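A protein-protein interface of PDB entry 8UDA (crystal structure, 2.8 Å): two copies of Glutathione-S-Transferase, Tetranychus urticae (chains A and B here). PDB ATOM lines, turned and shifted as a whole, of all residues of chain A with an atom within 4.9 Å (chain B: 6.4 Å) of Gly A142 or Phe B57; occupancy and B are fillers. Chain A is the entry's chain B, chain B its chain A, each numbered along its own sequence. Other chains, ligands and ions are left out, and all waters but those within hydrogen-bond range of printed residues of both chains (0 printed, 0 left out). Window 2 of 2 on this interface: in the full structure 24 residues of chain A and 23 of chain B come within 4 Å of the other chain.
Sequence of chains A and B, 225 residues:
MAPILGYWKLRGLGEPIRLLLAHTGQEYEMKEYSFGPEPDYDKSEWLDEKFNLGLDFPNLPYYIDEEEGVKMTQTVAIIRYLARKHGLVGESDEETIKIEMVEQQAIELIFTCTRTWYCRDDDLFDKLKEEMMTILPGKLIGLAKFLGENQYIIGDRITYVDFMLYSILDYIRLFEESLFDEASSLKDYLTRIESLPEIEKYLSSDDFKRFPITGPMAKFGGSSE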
ATOM      1  N   MET A 101      -9.501 -21.291 -12.264  1.00  0.00           N
ATOM      2  CA  MET A 101      -8.081 -21.276 -11.964  1.00  0.00           C
ATOM      3  C   MET A 101      -7.688 -22.632 -11.378  1.00  0.00           C
ATOM      4  O   MET A 101      -6.716 -23.238 -11.818  1.00  0.00           O
ATOM      5  CB  MET A 101      -7.731 -20.154 -10.978  1.00  0.00           C
ATOM      6  CG  MET A 101      -7.452 -18.824 -11.652  1.00  0.00           C
ATOM      7  SD  MET A 101      -6.852 -17.488 -10.557  1.00  0.00           S
ATOM      8  CE  MET A 101      -8.093 -17.441  -9.271  1.00  0.00           C
ATOM      9  N   VAL A 102      -8.466 -23.120 -10.402  1.00  0.00           N
ATOM     10  CA  VAL A 102      -8.135 -24.390  -9.767  1.00  0.00           C
ATOM     11  C   VAL A 102      -8.234 -25.518 -10.797  1.00  0.00           C
ATOM     12  O   VAL A 102      -7.381 -26.410 -10.814  1.00  0.00           O
ATOM     13  CB  VAL A 102      -8.979 -24.703  -8.516  1.00  0.00           C
ATOM     14  CG1 VAL A 102      -8.419 -25.884  -7.757  1.00  0.00           C
ATOM     15  CG2 VAL A 102      -9.067 -23.536  -7.563  1.00  0.00           C
ATOM     16  N   GLN A 105      -5.195 -25.518 -12.787  1.00  0.00           N
ATOM     17  CA  GLN A 105      -4.116 -25.889 -11.878  1.00  0.00           C
ATOM     18  C   GLN A 105      -4.019 -27.411 -11.769  1.00  0.00           C
ATOM     19  O   GLN A 105      -2.924 -27.966 -11.872  1.00  0.00           O
ATOM     20  CB  GLN A 105      -4.243 -25.139 -10.545  1.00  0.00           C
ATOM     21  CG  GLN A 105      -3.052 -25.307  -9.622  1.00  0.00           C
ATOM     22  CD  GLN A 105      -1.781 -24.770 -10.226  1.00  0.00           C
ATOM     23  OE1 GLN A 105      -1.686 -23.592 -10.556  1.00  0.00           O
ATOM     24  NE2 GLN A 105      -0.798 -25.642 -10.399  1.00  0.00           N
ATOM     25  N   GLY A 138       6.261 -26.558  -4.464  1.00  0.00           N
ATOM     26  CA  GLY A 138       5.735 -25.223  -4.715  1.00  0.00           C
ATOM     27  C   GLY A 138       4.249 -25.261  -5.074  1.00  0.00           C
ATOM     28  O   GLY A 138       3.461 -24.484  -4.538  1.00  0.00           O
ATOM     29  N   LYS A 139       3.891 -26.205  -5.959  1.00  0.00           N
ATOM     30  CA  LYS A 139       2.546 -26.353  -6.497  1.00  0.00           C
ATOM     31  C   LYS A 139       1.572 -26.657  -5.365  1.00  0.00           C
ATOM     32  O   LYS A 139       0.524 -26.024  -5.257  1.00  0.00           O
ATOM     33  CB  LYS A 139       2.484 -27.487  -7.528  1.00  0.00           C
ATOM     34  CG  LYS A 139       3.239 -27.244  -8.824  1.00  0.00           C
ATOM     35  CD  LYS A 139       2.878 -25.894  -9.404  1.00  0.00           C
ATOM     36  CE  LYS A 139       3.652 -25.561 -10.658  1.00  0.00           C
ATOM     37  NZ  LYS A 139       3.536 -24.123 -10.976  1.00  0.00           N
ATOM     38  N   LEU A 140       1.948 -27.629  -4.528  1.00  0.00           N
ATOM     39  CA  LEU A 140       1.121 -28.112  -3.438  1.00  0.00           C
ATOM     40  C   LEU A 140       0.936 -27.037  -2.372  1.00  0.00           C
ATOM     41  O   LEU A 140      -0.138 -26.931  -1.785  1.00  0.00           O
ATOM     42  CB  LEU A 140       1.760 -29.386  -2.873  1.00  0.00           C
ATOM     43  CG  LEU A 140       1.740 -30.552  -3.860  1.00  0.00           C
ATOM     44  CD1 LEU A 140       2.816 -31.571  -3.544  1.00  0.00           C
ATOM     45  CD2 LEU A 140       0.371 -31.205  -3.873  1.00  0.00           C
ATOM     46  N   ILE A 141       1.984 -26.241  -2.135  1.00  0.00           N
ATOM     47  CA  ILE A 141       1.908 -25.127  -1.201  1.00  0.00           C
ATOM     48  C   ILE A 141       0.920 -24.083  -1.727  1.00  0.00           C
ATOM     49  O   ILE A 141       0.090 -23.592  -0.971  1.00  0.00           O
ATOM     50  CB  ILE A 141       3.304 -24.540  -0.908  1.00  0.00           C
ATOM     51  CG1 ILE A 141       4.190 -25.572  -0.204  1.00  0.00           C
ATOM     52  CG2 ILE A 141       3.200 -23.251  -0.107  1.00  0.00           C
ATOM     53  CD1 ILE A 141       5.652 -25.208  -0.141  1.00  0.00           C
ATOM     54  N   GLY A 142       1.009 -23.760  -3.020  1.00  0.00           N
ATOM     55  CA  GLY A 142       0.072 -22.852  -3.659  1.00  0.00           C
ATOM     56  C   GLY A 142      -1.386 -23.256  -3.436  1.00  0.00           C
ATOM     57  O   GLY A 142      -2.230 -22.402  -3.181  1.00  0.00           O
ATOM     58  N   LEU A 143      -1.679 -24.560  -3.552  1.00  0.00           N
ATOM     59  CA  LEU A 143      -3.029 -25.067  -3.364  1.00  0.00           C
ATOM     60  C   LEU A 143      -3.399 -25.013  -1.886  1.00  0.00           C
ATOM     61  O   LEU A 143      -4.523 -24.658  -1.527  1.00  0.00           O
ATOM     62  CB  LEU A 143      -3.107 -26.501  -3.891  1.00  0.00           C
ATOM     63  CG  LEU A 143      -3.093 -26.639  -5.411  1.00  0.00           C
ATOM     64  CD1 LEU A 143      -3.005 -28.099  -5.833  1.00  0.00           C
ATOM     65  CD2 LEU A 143      -4.328 -25.989  -6.022  1.00  0.00           C
ATOM     66  N   ALA A 144      -2.434 -25.380  -1.039  1.00  0.00           N
ATOM     67  CA  ALA A 144      -2.614 -25.284   0.394  1.00  0.00           C
ATOM     68  C   ALA A 144      -3.003 -23.849   0.759  1.00  0.00           C
ATOM     69  O   ALA A 144      -3.995 -23.644   1.460  1.00  0.00           O
ATOM     70  CB  ALA A 144      -1.360 -25.747   1.078  1.00  0.00           C
ATOM     71  N   LYS A 145      -2.255 -22.863   0.236  1.00  0.00           N
ATOM     72  CA  LYS A 145      -2.520 -21.452   0.497  1.00  0.00           C
ATOM     73  C   LYS A 145      -3.908 -21.100  -0.014  1.00  0.00           C
ATOM     74  O   LYS A 145      -4.640 -20.419   0.697  1.00  0.00           O
ATOM     75  CB  LYS A 145      -1.544 -20.492  -0.192  1.00  0.00           C
ATOM     76  CG  LYS A 145      -0.065 -20.666   0.105  1.00  0.00           C
ATOM     77  CD  LYS A 145       0.294 -20.259   1.499  1.00  0.00           C
ATOM     78  CE  LYS A 145       1.782 -20.293   1.755  1.00  0.00           C
ATOM     79  NZ  LYS A 145       2.132 -19.428   2.903  1.00  0.00           N
ATOM     80  N   PHE A 146      -4.258 -21.598  -1.212  1.00  0.00           N
ATOM     81  CA  PHE A 146      -5.535 -21.276  -1.827  1.00  0.00           C
ATOM     82  C   PHE A 146      -6.671 -21.751  -0.928  1.00  0.00           C
ATOM     83  O   PHE A 146      -7.594 -20.993  -0.622  1.00  0.00           O
ATOM     84  CB  PHE A 146      -5.722 -21.889  -3.222  1.00  0.00           C
ATOM     85  CG  PHE A 146      -6.872 -21.232  -3.949  1.00  0.00           C
ATOM     86  CD1 PHE A 146      -6.826 -19.875  -4.300  1.00  0.00           C
ATOM     87  CD2 PHE A 146      -8.019 -21.945  -4.282  1.00  0.00           C
ATOM     88  CE1 PHE A 146      -7.884 -19.248  -4.953  1.00  0.00           C
ATOM     89  CE2 PHE A 146      -9.075 -21.317  -4.944  1.00  0.00           C
ATOM     90  CZ  PHE A 146      -9.019 -19.968  -5.273  1.00  0.00           C
ATOM     91  N   LEU B  55      -1.165 -12.926  -6.610  1.00  0.00           N
ATOM     92  CA  LEU B  55      -1.733 -13.956  -7.471  1.00  0.00           C
ATOM     93  C   LEU B  55      -1.868 -15.249  -6.669  1.00  0.00           C
ATOM     94  O   LEU B  55      -0.907 -15.706  -6.054  1.00  0.00           O
ATOM     95  CB  LEU B  55      -0.817 -14.166  -8.685  1.00  0.00           C
ATOM     96  CG  LEU B  55      -0.509 -12.935  -9.550  1.00  0.00           C
ATOM     97  CD1 LEU B  55       0.625 -13.240 -10.529  1.00  0.00           C
ATOM     98  CD2 LEU B  55      -1.750 -12.440 -10.293  1.00  0.00           C
ATOM     99  N   ASP B  56      -3.077 -15.819  -6.667  1.00  0.00           N
ATOM    100  CA  ASP B  56      -3.319 -17.117  -6.051  1.00  0.00           C
ATOM    101  C   ASP B  56      -2.344 -18.176  -6.578  1.00  0.00           C
ATOM    102  O   ASP B  56      -1.723 -18.873  -5.784  1.00  0.00           O
ATOM    103  CB  ASP B  56      -4.787 -17.527  -6.144  1.00  0.00           C
ATOM    104  CG  ASP B  56      -5.695 -16.787  -5.174  1.00  0.00           C
ATOM    105  OD1 ASP B  56      -5.434 -16.841  -3.935  1.00  0.00           O
ATOM    106  OD2 ASP B  56      -6.688 -16.193  -5.653  1.00  0.00           O
ATOM    107  N   PHE B  57      -2.204 -18.291  -7.905  1.00  0.00           N
ATOM    108  CA  PHE B  57      -1.277 -19.242  -8.516  1.00  0.00           C
ATOM    109  C   PHE B  57      -0.303 -18.490  -9.411  1.00  0.00           C
ATOM    110  O   PHE B  57      -0.459 -18.502 -10.626  1.00  0.00           O
ATOM    111  CB  PHE B  57      -2.010 -20.346  -9.286  1.00  0.00           C
ATOM    112  CG  PHE B  57      -2.988 -21.060  -8.403  1.00  0.00           C
ATOM    113  CD1 PHE B  57      -2.524 -21.845  -7.361  1.00  0.00           C
ATOM    114  CD2 PHE B  57      -4.351 -20.842  -8.537  1.00  0.00           C
ATOM    115  CE1 PHE B  57      -3.416 -22.465  -6.501  1.00  0.00           C
ATOM    116  CE2 PHE B  57      -5.244 -21.451  -7.670  1.00  0.00           C
ATOM    117  CZ  PHE B  57      -4.776 -22.272  -6.664  1.00  0.00           C
ATOM    118  N   PRO B  58       0.709 -17.795  -8.839  1.00  0.00           N
ATOM    119  CA  PRO B  58       1.577 -16.922  -9.626  1.00  0.00           C
ATOM    120  C   PRO B  58       2.160 -17.766 -10.758  1.00  0.00           C
ATOM    121  O   PRO B  58       2.752 -18.827 -10.535  1.00  0.00           O
ATOM    122  CB  PRO B  58       2.622 -16.439  -8.610  1.00  0.00           C
ATOM    123  CG  PRO B  58       2.581 -17.483  -7.532  1.00  0.00           C
ATOM    124  CD  PRO B  58       1.119 -17.867  -7.430  1.00  0.00           C
ATOM    125  N   ASN B  59       1.932 -17.277 -11.978  1.00  0.00           N
ATOM    126  CA  ASN B  59       2.333 -17.956 -13.189  1.00  0.00           C
ATOM    127  C   ASN B  59       2.127 -16.971 -14.326  1.00  0.00           C
ATOM    128  O   ASN B  59       1.383 -16.003 -14.154  1.00  0.00           O
ATOM    129  CB  ASN B  59       1.486 -19.208 -13.424  1.00  0.00           C
ATOM    130  CG  ASN B  59       2.193 -20.225 -14.283  1.00  0.00           C
ATOM    131  OD1 ASN B  59       3.221 -19.929 -14.887  1.00  0.00           O
ATOM    132  ND2 ASN B  59       1.680 -21.442 -14.275  1.00  0.00           N
ATOM    133  N   LEU B  60       2.789 -17.235 -15.464  1.00  0.00           N
ATOM    134  CA  LEU B  60       2.574 -16.468 -16.684  1.00  0.00           C
ATOM    135  C   LEU B  60       1.807 -17.330 -17.689  1.00  0.00           C
ATOM    136  O   LEU B  60       2.195 -18.463 -17.973  1.00  0.00           O
ATOM    137  CB  LEU B  60       3.926 -16.002 -17.240  1.00  0.00           C
ATOM    138  CG  LEU B  60       4.613 -14.852 -16.503  1.00  0.00           C
ATOM    139  CD1 LEU B  60       5.860 -14.397 -17.244  1.00  0.00           C
ATOM    140  CD2 LEU B  60       3.674 -13.676 -16.354  1.00  0.00           C
ATOM    141  N   PRO B  61       0.691 -16.838 -18.267  1.00  0.00           N
ATOM    142  CA  PRO B  61       0.317 -15.428 -18.148  1.00  0.00           C
ATOM    143  C   PRO B  61      -0.495 -15.100 -16.889  1.00  0.00           C
ATOM    144  O   PRO B  61      -0.948 -16.006 -16.185  1.00  0.00           O
ATOM    145  CB  PRO B  61      -0.557 -15.277 -19.395  1.00  0.00           C
ATOM    146  CG  PRO B  61      -1.287 -16.606 -19.507  1.00  0.00           C
ATOM    147  CD  PRO B  61      -0.296 -17.644 -19.016  1.00  0.00           C
ATOM    148  N   MET B  72      -6.029 -12.813 -11.939  1.00  0.00           N
ATOM    149  CA  MET B  72      -6.136 -14.219 -12.319  1.00  0.00           C
ATOM    150  C   MET B  72      -4.792 -14.667 -12.880  1.00  0.00           C
ATOM    151  O   MET B  72      -3.975 -13.789 -13.172  1.00  0.00           O
ATOM    152  CB  MET B  72      -7.143 -14.342 -13.457  1.00  0.00           C
ATOM    153  CG  MET B  72      -8.523 -13.943 -13.076  1.00  0.00           C
ATOM    154  SD  MET B  72      -9.566 -14.031 -14.534  1.00  0.00           S
ATOM    155  CE  MET B  72      -9.896 -15.791 -14.599  1.00  0.00           C
ATOM    156  N   THR B  73      -4.608 -15.992 -13.093  1.00  0.00           N
ATOM    157  CA  THR B  73      -3.311 -16.491 -13.528  1.00  0.00           C
ATOM    158  C   THR B  73      -3.369 -17.677 -14.493  1.00  0.00           C
ATOM    159  O   THR B  73      -2.305 -18.122 -14.930  1.00  0.00           O
ATOM    160  CB  THR B  73      -2.436 -16.944 -12.355  1.00  0.00           C
ATOM    161  OG1 THR B  73      -2.940 -18.200 -11.898  1.00  0.00           O
ATOM    162  CG2 THR B  73      -2.444 -15.973 -11.196  1.00  0.00           C
ATOM    163  N   GLN B  74      -4.552 -18.211 -14.828  1.00  0.00           N
ATOM    164  CA  GLN B  74      -4.557 -19.383 -15.709  1.00  0.00           C
ATOM    165  C   GLN B  74      -5.084 -19.031 -17.107  1.00  0.00           C
ATOM    166  O   GLN B  74      -6.183 -18.491 -17.231  1.00  0.00           O
ATOM    167  CB  GLN B  74      -5.377 -20.536 -15.115  1.00  0.00           C
ATOM    168  CG  GLN B  74      -4.913 -20.975 -13.737  1.00  0.00           C
ATOM    169  CD  GLN B  74      -3.539 -21.585 -13.818  1.00  0.00           C
ATOM    170  OE1 GLN B  74      -3.305 -22.514 -14.597  1.00  0.00           O
ATOM    171  NE2 GLN B  74      -2.623 -21.033 -13.031  1.00  0.00           N
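SD of Met A101 touches CA of Met B72 (3.8 Å).
Met A101 touches Gln B74 (O to CG, 3.5 Å).
OE1 of Gln A105 touches CB of Phe B57, at 3.5 Å.
OE1 of Gln A105 touches NE2 of Gln B74 (3.7 Å).
Gly A142 touches Phe B57 (O to CE1, 3.5 Å).
CE1 of Phe B57 touches CD2 of Leu A143, 3.7 Å away.
Phe A146 touches Asp B56.
Phe B57 touches Phe A146.
The backbone NH (N) of Thr B73 sits at hydrogen-bond distance from the side-chain sulfur (SD) of Met A101 (3.7 Å).
O of Phe B57 sits at hydrogen-bond distance from OG1 of Thr B73 (2.8 Å).
OG1 of Thr B73 sits at hydrogen-bond distance from NE2 of Gln B74, at 3.1 Å.
Printed residues of chain B within 4 Å of Gln A105: Phe B57 and Gln B74.
Lys A139 touches none of the printed residues of chain B.
Gly A142 touches just one residue of chain B: Phe B57.
Printed residues of chain B within 4 Å of Leu A143: Phe B57.
Leu B55 touches none of the printed residues of chain A.
Printed residues of chain A within 4 Å of Asp B56: Phe A146 (3.3 Å).
Of chain A, only Gln A105 (3.5 Å), Gly A142 (3.5 Å), Leu A143 (3.7 Å) and Phe A146 (3.6 Å) come within 4 Å of Phe B57.
Printed residues of chain A within 4 Å of Met B72: Met A101 (3.8 Å).
Printed residues of chain A within 4 Å of Thr B73: Met A101.
The nearest residue of chain A that does not touch Phe B57 is Met A101 (4.2 Å).
The nearest printed residue of chain B that does not touch Phe A146 is Leu B55 (7.2 Å).
No position is printed for both chains.
Of the 9 pairs that touch across the chains among the printed residues, none has its exchanged pair printed and touching as well.
Of the 12 printed residues of chain A, 5 touch a printed residue of chain B.
Of the 10 printed residues of chain B, 5 touch a printed residue of chain A.
Printed residues of chain B that touch a printed residue of chain A: Asp B56, Phe B57, Met B72, Thr B73 and Gln B74.
Among the printed residues, 9 pairs touch across the chains.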
